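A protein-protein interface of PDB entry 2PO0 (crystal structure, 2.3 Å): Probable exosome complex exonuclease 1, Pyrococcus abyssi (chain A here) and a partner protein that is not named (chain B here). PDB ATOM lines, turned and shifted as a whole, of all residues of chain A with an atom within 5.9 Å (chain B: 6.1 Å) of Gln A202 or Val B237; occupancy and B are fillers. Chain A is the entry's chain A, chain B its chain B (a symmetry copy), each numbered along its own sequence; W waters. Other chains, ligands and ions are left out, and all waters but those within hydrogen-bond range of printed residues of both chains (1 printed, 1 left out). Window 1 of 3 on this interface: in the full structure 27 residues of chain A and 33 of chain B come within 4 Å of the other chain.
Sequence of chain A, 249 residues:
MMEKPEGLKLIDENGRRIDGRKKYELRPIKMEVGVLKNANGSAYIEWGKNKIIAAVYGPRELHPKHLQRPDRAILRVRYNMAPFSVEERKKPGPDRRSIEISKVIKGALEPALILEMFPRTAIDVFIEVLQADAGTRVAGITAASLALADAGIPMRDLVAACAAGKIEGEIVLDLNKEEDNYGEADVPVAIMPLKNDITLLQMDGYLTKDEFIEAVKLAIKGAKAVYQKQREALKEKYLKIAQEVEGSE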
ATOM      1  N   GLU A 100      -0.575  23.828   3.759  1.00  0.00           N
ATOM      2  CA  GLU A 100       0.757  23.640   3.243  1.00  0.00           C
ATOM      3  C   GLU A 100       1.594  22.710   4.136  1.00  0.00           C
ATOM      4  O   GLU A 100       2.345  21.882   3.641  1.00  0.00           O
ATOM      5  CB  GLU A 100       1.489  24.973   3.010  1.00  0.00           C
ATOM      6  CG  GLU A 100       2.977  24.720   2.490  1.00  0.00           C
ATOM      7  CD  GLU A 100       4.023  25.844   2.664  1.00  0.00           C
ATOM      8  OE1 GLU A 100       3.754  26.894   3.254  1.00  0.00           O
ATOM      9  OE2 GLU A 100       5.170  25.646   2.218  1.00  0.00           O
ATOM     10  N   VAL A 104       3.366  18.876   3.392  1.00  0.00           N
ATOM     11  CA  VAL A 104       4.822  18.737   3.514  1.00  0.00           C
ATOM     12  C   VAL A 104       5.126  17.707   4.606  1.00  0.00           C
ATOM     13  O   VAL A 104       6.134  17.009   4.559  1.00  0.00           O
ATOM     14  CB  VAL A 104       5.374  20.235   3.681  1.00  0.00           C
ATOM     15  CG1 VAL A 104       5.764  20.714   5.120  1.00  0.00           C
ATOM     16  CG2 VAL A 104       6.164  20.730   2.512  1.00  0.00           C
ATOM     17  N   ARG A 137       5.880  22.114  13.054  1.00  0.00           N
ATOM     18  CA  ARG A 137       5.745  21.173  11.931  1.00  0.00           C
ATOM     19  C   ARG A 137       6.720  20.049  12.167  1.00  0.00           C
ATOM     20  O   ARG A 137       6.351  18.880  12.056  1.00  0.00           O
ATOM     21  CB  ARG A 137       5.905  21.815  10.547  1.00  0.00           C
ATOM     22  CG  ARG A 137       7.339  21.934  10.056  1.00  0.00           C
ATOM     23  CD  ARG A 137       7.374  22.847   8.883  1.00  0.00           C
ATOM     24  NE  ARG A 137       6.818  24.152   9.207  1.00  0.00           N
ATOM     25  CZ  ARG A 137       6.453  25.052   8.298  1.00  0.00           C
ATOM     26  NH1 ARG A 137       6.553  24.743   7.017  1.00  0.00           N
ATOM     27  NH2 ARG A 137       5.917  26.212   8.662  1.00  0.00           N
ATOM     28  N   ASP A 186      14.428  30.368   8.767  1.00  0.00           N
ATOM     29  CA  ASP A 186      13.942  29.218   9.458  1.00  0.00           C
ATOM     30  C   ASP A 186      14.054  28.066   8.442  1.00  0.00           C
ATOM     31  O   ASP A 186      13.481  28.127   7.356  1.00  0.00           O
ATOM     32  CB  ASP A 186      12.485  29.491   9.833  1.00  0.00           C
ATOM     33  CG  ASP A 186      11.833  28.388  10.657  1.00  0.00           C
ATOM     34  OD1 ASP A 186      10.575  28.476  10.757  1.00  0.00           O
ATOM     35  OD2 ASP A 186      12.487  27.475  11.214  1.00  0.00           O
ATOM     36  N   VAL A 187      14.797  27.027   8.803  1.00  0.00           N
ATOM     37  CA  VAL A 187      15.081  25.888   7.909  1.00  0.00           C
ATOM     38  C   VAL A 187      14.594  24.626   8.604  1.00  0.00           C
ATOM     39  O   VAL A 187      15.340  24.032   9.349  1.00  0.00           O
ATOM     40  CB  VAL A 187      16.636  25.786   7.568  1.00  0.00           C
ATOM     41  CG1 VAL A 187      16.909  24.765   6.491  1.00  0.00           C
ATOM     42  CG2 VAL A 187      17.156  27.120   7.121  1.00  0.00           C
ATOM     43  N   PRO A 188      13.308  24.250   8.433  1.00  0.00           N
ATOM     44  CA  PRO A 188      12.967  22.930   8.987  1.00  0.00           C
ATOM     45  C   PRO A 188      13.529  21.787   8.157  1.00  0.00           C
ATOM     46  O   PRO A 188      13.495  21.847   6.933  1.00  0.00           O
ATOM     47  CB  PRO A 188      11.449  22.909   8.933  1.00  0.00           C
ATOM     48  CG  PRO A 188      11.083  23.968   8.033  1.00  0.00           C
ATOM     49  CD  PRO A 188      12.135  24.923   7.843  1.00  0.00           C
ATOM     50  N   VAL A 189      14.040  20.754   8.818  1.00  0.00           N
ATOM     51  CA  VAL A 189      14.438  19.543   8.107  1.00  0.00           C
ATOM     52  C   VAL A 189      13.761  18.333   8.757  1.00  0.00           C
ATOM     53  O   VAL A 189      13.531  18.331   9.971  1.00  0.00           O
ATOM     54  CB  VAL A 189      16.002  19.414   8.038  1.00  0.00           C
ATOM     55  CG1 VAL A 189      16.439  18.192   7.260  1.00  0.00           C
ATOM     56  CG2 VAL A 189      16.645  20.700   7.419  1.00  0.00           C
ATOM     57  N   LEU A 200      11.870  16.160   4.500  1.00  0.00           N
ATOM     58  CA  LEU A 200      11.368  17.509   4.561  1.00  0.00           C
ATOM     59  C   LEU A 200      12.517  18.525   4.482  1.00  0.00           C
ATOM     60  O   LEU A 200      13.517  18.442   5.187  1.00  0.00           O
ATOM     61  CB  LEU A 200      10.547  17.744   5.836  1.00  0.00           C
ATOM     62  CG  LEU A 200       9.959  19.182   5.988  1.00  0.00           C
ATOM     63  CD1 LEU A 200       8.443  19.206   6.244  1.00  0.00           C
ATOM     64  CD2 LEU A 200      10.685  20.052   6.987  1.00  0.00           C
ATOM     65  N   LEU A 201      12.386  19.511   3.629  1.00  0.00           N
ATOM     66  CA  LEU A 201      13.368  20.574   3.627  1.00  0.00           C
ATOM     67  C   LEU A 201      12.703  21.831   3.162  1.00  0.00           C
ATOM     68  O   LEU A 201      12.255  21.895   2.035  1.00  0.00           O
ATOM     69  CB  LEU A 201      14.544  20.248   2.704  1.00  0.00           C
ATOM     70  CG  LEU A 201      15.984  20.623   3.158  1.00  0.00           C
ATOM     71  CD1 LEU A 201      16.840  20.634   1.903  1.00  0.00           C
ATOM     72  CD2 LEU A 201      16.097  21.961   3.880  1.00  0.00           C
ATOM     73  N   GLN A 202      12.625  22.820   4.037  1.00  0.00           N
ATOM     74  CA  GLN A 202      12.108  24.141   3.668  1.00  0.00           C
ATOM     75  C   GLN A 202      13.010  25.206   4.257  1.00  0.00           C
ATOM     76  O   GLN A 202      13.679  25.005   5.242  1.00  0.00           O
ATOM     77  CB  GLN A 202      10.663  24.329   4.164  1.00  0.00           C
ATOM     78  CG  GLN A 202       9.703  23.174   3.943  1.00  0.00           C
ATOM     79  CD  GLN A 202       8.341  23.433   4.542  1.00  0.00           C
ATOM     80  OE1 GLN A 202       8.045  23.008   5.655  1.00  0.00           O
ATOM     81  NE2 GLN A 202       7.491  24.122   3.795  1.00  0.00           N
ATOM     82  N   MET A 203      13.046  26.338   3.599  1.00  0.00           N
ATOM     83  CA  MET A 203      13.765  27.492   4.028  1.00  0.00           C
ATOM     84  C   MET A 203      12.827  28.682   3.733  1.00  0.00           C
ATOM     85  O   MET A 203      12.217  28.831   2.653  1.00  0.00           O
ATOM     86  CB  MET A 203      15.095  27.602   3.263  1.00  0.00           C
ATOM     87  CG  MET A 203      16.139  28.537   3.846  1.00  0.00           C
ATOM     88  SD  MET A 203      15.764  30.259   3.444  1.00  0.00           S
ATOM     89  CE  MET A 203      15.396  30.185   1.745  1.00  0.00           C
ATOM     90  N   ASP A 204      12.713  29.517   4.742  1.00  0.00           N
ATOM     91  CA  ASP A 204      11.883  30.676   4.734  1.00  0.00           C
ATOM     92  C   ASP A 204      12.878  31.705   5.204  1.00  0.00           C
ATOM     93  O   ASP A 204      13.439  31.530   6.249  1.00  0.00           O
ATOM     94  CB  ASP A 204      10.824  30.465   5.817  1.00  0.00           C
ATOM     95  CG  ASP A 204       9.767  31.393   5.700  1.00  0.00           C
ATOM     96  OD1 ASP A 204       9.817  32.130   4.689  1.00  0.00           O
ATOM     97  OD2 ASP A 204       8.851  31.423   6.584  1.00  0.00           O
ATOM     98  N   PHE A 212      22.668  28.448   4.232  1.00  0.00           N
ATOM     99  CA  PHE A 212      21.679  27.403   4.012  1.00  0.00           C
ATOM    100  C   PHE A 212      22.206  26.029   4.403  1.00  0.00           C
ATOM    101  O   PHE A 212      21.636  25.422   5.284  1.00  0.00           O
ATOM    102  CB  PHE A 212      21.170  27.363   2.576  1.00  0.00           C
ATOM    103  CG  PHE A 212      20.164  26.274   2.349  1.00  0.00           C
ATOM    104  CD1 PHE A 212      20.385  25.305   1.382  1.00  0.00           C
ATOM    105  CD2 PHE A 212      19.018  26.197   3.132  1.00  0.00           C
ATOM    106  CE1 PHE A 212      19.482  24.308   1.161  1.00  0.00           C
ATOM    107  CE2 PHE A 212      18.104  25.180   2.930  1.00  0.00           C
ATOM    108  CZ  PHE A 212      18.338  24.232   1.935  1.00  0.00           C
ATOM    109  N   VAL B 112       5.037  29.273  -1.699  1.00  0.00           N
ATOM    110  CA  VAL B 112       6.426  29.205  -2.127  1.00  0.00           C
ATOM    111  C   VAL B 112       6.802  30.343  -3.073  1.00  0.00           C
ATOM    112  O   VAL B 112       7.836  30.928  -2.891  1.00  0.00           O
ATOM    113  CB  VAL B 112       6.798  27.783  -2.755  1.00  0.00           C
ATOM    114  CG1 VAL B 112       8.337  27.641  -3.091  1.00  0.00           C
ATOM    115  CG2 VAL B 112       6.313  26.618  -1.823  1.00  0.00           C
ATOM    116  N   ARG B 115       6.914  33.610  -1.127  1.00  0.00           N
ATOM    117  CA  ARG B 115       7.927  33.589  -0.114  1.00  0.00           C
ATOM    118  C   ARG B 115       9.268  33.952  -0.722  1.00  0.00           C
ATOM    119  O   ARG B 115       9.946  34.824  -0.224  1.00  0.00           O
ATOM    120  CB  ARG B 115       7.892  32.205   0.476  1.00  0.00           C
ATOM    121  CG  ARG B 115       8.848  31.868   1.561  1.00  0.00           C
ATOM    122  CD  ARG B 115       8.021  31.026   2.548  1.00  0.00           C
ATOM    123  NE  ARG B 115       7.924  29.666   2.065  1.00  0.00           N
ATOM    124  CZ  ARG B 115       6.859  28.869   2.209  1.00  0.00           C
ATOM    125  NH1 ARG B 115       6.935  27.669   1.694  1.00  0.00           N
ATOM    126  NH2 ARG B 115       5.757  29.242   2.859  1.00  0.00           N
ATOM    127  N   ILE B 224      12.537  19.160  -5.542  1.00  0.00           N
ATOM    128  CA  ILE B 224      13.039  20.147  -4.611  1.00  0.00           C
ATOM    129  C   ILE B 224      13.180  21.445  -5.368  1.00  0.00           C
ATOM    130  O   ILE B 224      13.673  21.407  -6.488  1.00  0.00           O
ATOM    131  CB  ILE B 224      14.344  19.718  -3.924  1.00  0.00           C
ATOM    132  CG1 ILE B 224      14.629  20.642  -2.715  1.00  0.00           C
ATOM    133  CG2 ILE B 224      15.521  19.561  -4.934  1.00  0.00           C
ATOM    134  CD1 ILE B 224      15.699  20.108  -1.799  1.00  0.00           C
ATOM    135  N   THR B 225      12.667  22.538  -4.793  1.00  0.00           N
ATOM    136  CA  THR B 225      12.754  23.877  -5.382  1.00  0.00           C
ATOM    137  C   THR B 225      13.656  24.802  -4.560  1.00  0.00           C
ATOM    138  O   THR B 225      13.577  24.847  -3.350  1.00  0.00           O
ATOM    139  CB  THR B 225      11.363  24.502  -5.623  1.00  0.00           C
ATOM    140  OG1 THR B 225      10.623  23.628  -6.496  1.00  0.00           O
ATOM    141  CG2 THR B 225      11.448  25.960  -6.243  1.00  0.00           C
ATOM    142  N   ILE B 226      14.598  25.430  -5.255  1.00  0.00           N
ATOM    143  CA  ILE B 226      15.528  26.418  -4.670  1.00  0.00           C
ATOM    144  C   ILE B 226      15.401  27.716  -5.424  1.00  0.00           C
ATOM    145  O   ILE B 226      15.633  27.771  -6.606  1.00  0.00           O
ATOM    146  CB  ILE B 226      16.987  25.903  -4.648  1.00  0.00           C
ATOM    147  CG1 ILE B 226      17.085  24.660  -3.740  1.00  0.00           C
ATOM    148  CG2 ILE B 226      17.942  26.997  -4.175  1.00  0.00           C
ATOM    149  CD1 ILE B 226      17.654  23.596  -4.401  1.00  0.00           C
ATOM    150  N   THR B 227      14.944  28.728  -4.721  1.00  0.00           N
ATOM    151  CA  THR B 227      14.736  30.067  -5.269  1.00  0.00           C
ATOM    152  C   THR B 227      15.859  31.042  -4.869  1.00  0.00           C
ATOM    153  O   THR B 227      16.078  31.302  -3.711  1.00  0.00           O
ATOM    154  CB  THR B 227      13.370  30.641  -4.802  1.00  0.00           C
ATOM    155  OG1 THR B 227      12.338  29.692  -5.104  1.00  0.00           O
ATOM    156  CG2 THR B 227      13.085  32.040  -5.429  1.00  0.00           C
ATOM    157  N   ILE B 234      19.612  32.846  -1.209  1.00  0.00           N
ATOM    158  CA  ILE B 234      18.468  31.971  -1.353  1.00  0.00           C
ATOM    159  C   ILE B 234      17.338  32.580  -0.525  1.00  0.00           C
ATOM    160  O   ILE B 234      17.527  32.923   0.625  1.00  0.00           O
ATOM    161  CB  ILE B 234      18.809  30.498  -0.872  1.00  0.00           C
ATOM    162  CG1 ILE B 234      20.165  29.995  -1.459  1.00  0.00           C
ATOM    163  CG2 ILE B 234      17.693  29.569  -1.229  1.00  0.00           C
ATOM    164  CD1 ILE B 234      20.827  28.900  -0.646  1.00  0.00           C
ATOM    165  N   SER B 235      16.167  32.710  -1.119  1.00  0.00           N
ATOM    166  CA  SER B 235      15.006  33.258  -0.417  1.00  0.00           C
ATOM    167  C   SER B 235      13.863  32.256  -0.263  1.00  0.00           C
ATOM    168  O   SER B 235      12.825  32.626   0.289  1.00  0.00           O
ATOM    169  CB  SER B 235      14.477  34.504  -1.147  1.00  0.00           C
ATOM    170  OG  SER B 235      13.996  34.175  -2.454  1.00  0.00           O
ATOM    171  N   ALA B 236      14.020  31.025  -0.784  1.00  0.00           N
ATOM    172  CA  ALA B 236      13.112  29.869  -0.515  1.00  0.00           C
ATOM    173  C   ALA B 236      13.668  28.573  -1.030  1.00  0.00           C
ATOM    174  O   ALA B 236      14.184  28.500  -2.146  1.00  0.00           O
ATOM    175  CB  ALA B 236      11.692  30.057  -1.094  1.00  0.00           C
ATOM    176  N   VAL B 237      13.527  27.558  -0.184  1.00  0.00           N
ATOM    177  CA  VAL B 237      13.748  26.146  -0.490  1.00  0.00           C
ATOM    178  C   VAL B 237      12.447  25.422  -0.067  1.00  0.00           C
ATOM    179  O   VAL B 237      11.823  25.754   0.948  1.00  0.00           O
ATOM    180  CB  VAL B 237      14.985  25.595   0.269  1.00  0.00           C
ATOM    181  CG1 VAL B 237      15.216  24.088   0.014  1.00  0.00           C
ATOM    182  CG2 VAL B 237      16.213  26.449  -0.044  1.00  0.00           C
ATOM    183  N   GLN B 238      12.047  24.460  -0.893  1.00  0.00           N
ATOM    184  CA  GLN B 238      10.869  23.633  -0.742  1.00  0.00           C
ATOM    185  C   GLN B 238      11.139  22.288  -1.427  1.00  0.00           C
ATOM    186  O   GLN B 238      11.162  22.178  -2.629  1.00  0.00           O
ATOM    187  CB  GLN B 238       9.655  24.325  -1.394  1.00  0.00           C
ATOM    188  CG  GLN B 238       8.316  23.655  -1.108  1.00  0.00           C
ATOM    189  CD  GLN B 238       7.716  24.026   0.222  1.00  0.00           C
ATOM    190  OE1 GLN B 238       8.358  24.654   1.073  1.00  0.00           O
ATOM    191  NE2 GLN B 238       6.468  23.625   0.424  1.00  0.00           N
ATOM    192  N   LYS B 239      11.343  21.274  -0.625  1.00  0.00           N
ATOM    193  CA  LYS B 239      11.223  19.919  -1.067  1.00  0.00           C
ATOM    194  C   LYS B 239       9.729  19.645  -1.027  1.00  0.00           C
ATOM    195  O   LYS B 239       9.030  19.970  -0.023  1.00  0.00           O
ATOM    196  CB  LYS B 239      12.013  18.961  -0.145  1.00  0.00           C
ATOM    197  CG  LYS B 239      11.891  17.476  -0.484  1.00  0.00           C
ATOM    198  CD  LYS B 239      10.625  16.839   0.042  1.00  0.00           C
ATOM    199  CE  LYS B 239      10.626  15.400  -0.329  1.00  0.00           C
ATOM    200  NZ  LYS B 239       9.639  14.653   0.471  1.00  0.00           N
ATOM    201  N   VAL B 250      21.126  17.932  -2.318  1.00  0.00           N
ATOM    202  CA  VAL B 250      20.723  19.271  -1.912  1.00  0.00           C
ATOM    203  C   VAL B 250      21.783  20.326  -2.234  1.00  0.00           C
ATOM    204  O   VAL B 250      21.470  21.328  -2.868  1.00  0.00           O
ATOM    205  CB  VAL B 250      20.245  19.332  -0.419  1.00  0.00           C
ATOM    206  CG1 VAL B 250      19.914  20.795  -0.002  1.00  0.00           C
ATOM    207  CG2 VAL B 250      19.053  18.341  -0.202  1.00  0.00           C
ATOM    208  N   VAL B 254      21.238  23.399  -5.035  1.00  0.00           N
ATOM    209  CA  VAL B 254      21.493  24.784  -4.687  1.00  0.00           C
ATOM    210  C   VAL B 254      22.445  25.464  -5.701  1.00  0.00           C
ATOM    211  O   VAL B 254      22.122  26.523  -6.279  1.00  0.00           O
ATOM    212  CB  VAL B 254      21.989  24.865  -3.225  1.00  0.00           C
ATOM    213  CG1 VAL B 254      22.660  26.178  -2.961  1.00  0.00           C
ATOM    214  CG2 VAL B 254      20.785  24.635  -2.246  1.00  0.00           C
HETATM  215  O   HOH W   1       9.594  19.718   2.542  1.00  0.00           O
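The side-chain carboxylate (OE2) of Glu A100 is in salt-bridge range of the guanidinium group (NH1) of Arg B115 (2.7 Å).
OE2 of Glu A100 lies within hydrogen-bond range of NE2 of Gln B238 (3.0 Å).
O of Leu A201 is in hydrogen-bond range of N of Lys B239.
The side-chain amide nitrogen (NE2) of Gln A202 is in hydrogen-bond range of the side-chain amide oxygen (OE1) of Gln B238, 2.9 Å away.
N of Met A203 lies within hydrogen-bond range of O of Val B237 (3.0 Å).
The side-chain carboxylate (OE2) of Glu A100 lies within hydrogen-bond range of the side-chain amide nitrogen (NE2) of Gln A202 (3.2 Å).
OE1 of Gln A202 sits at hydrogen-bond distance from NH1 of Arg A137 (2.7 Å).
N of Asp A186 is in hydrogen-bond range of O of Asp A204.
The side-chain amide oxygen of Gln B238 lies within hydrogen-bond range of the guanidinium group of Arg B115 (3.4 Å).
The backbone carbonyl oxygen of Thr B227 is in hydrogen-bond range of the backbone NH of Ser B235, 3.0 Å away.
The backbone NH of Thr B227 is in hydrogen-bond range of the backbone carbonyl oxygen of Ala B236 (2.7 Å).
NE2 of Gln B238 touches CG2 of Val A104, 3.6 Å away.
Lys B239 touches Val A104 (O to CG2, 3.9 Å).
CD1 of Leu A201 touches CD1 of Ile B224, 3.9 Å away.
Leu A201 touches Gln B238 (O to CA, 3.6 Å).
O of Val B237 touches CA of Gln A202 (3.2 Å).
O of Ile B234 touches CE of Met A203 (3.6 Å).
Asp A204 touches Arg B115.
Ile B234 touches Phe A212 (CD1 to CB, 3.6 Å).
Phe A212 touches Val B237.
Phe A212 touches Val B250.
Of the printed residues of chain B, Leu A201 touches Ile B224 (3.9 Å), Gln B238 (3.6 Å), Lys B239 (2.9 Å) and Val B250 (3.6 Å).
Of the printed residues of chain B, Gln A202 touches Val B237 and Gln B238.
Of chain A, only Gln A202, Met A203 and Phe A212 come within 4 Å of Val B237.
Of the printed residues of chain A, Val B250 touches Leu A201 (3.6 Å) and Phe A212 (3.7 Å).
The nearest residue of chain A that does not touch Val B237 is Leu A201 (4.03 Å).
The nearest printed residue of chain A that does not touch Ser B235 is Asp A204 (4.9 Å).
Of the 14 printed residues of chain B, 10 touch a printed residue of chain A.
Hydrophobic or aromatic side chains of chain B that line the printed part of chain A: Ile B224, Ile B234, Ala B236, Val B237, Val B250 and Val B254.
Of the 13 printed residues of chain A, 7 touch a printed residue of chain B.
Printed residues of chain A that touch a printed residue of chain B: Glu A100, Val A104, Leu A201, Gln A202, Met A203, Asp A204 and Phe A212.
Among the printed residues, 19 pairs touch across the chains.
Water W1 bridges the backbone carbonyl oxygen of Lys B239 and the backbone NH of Leu A201.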
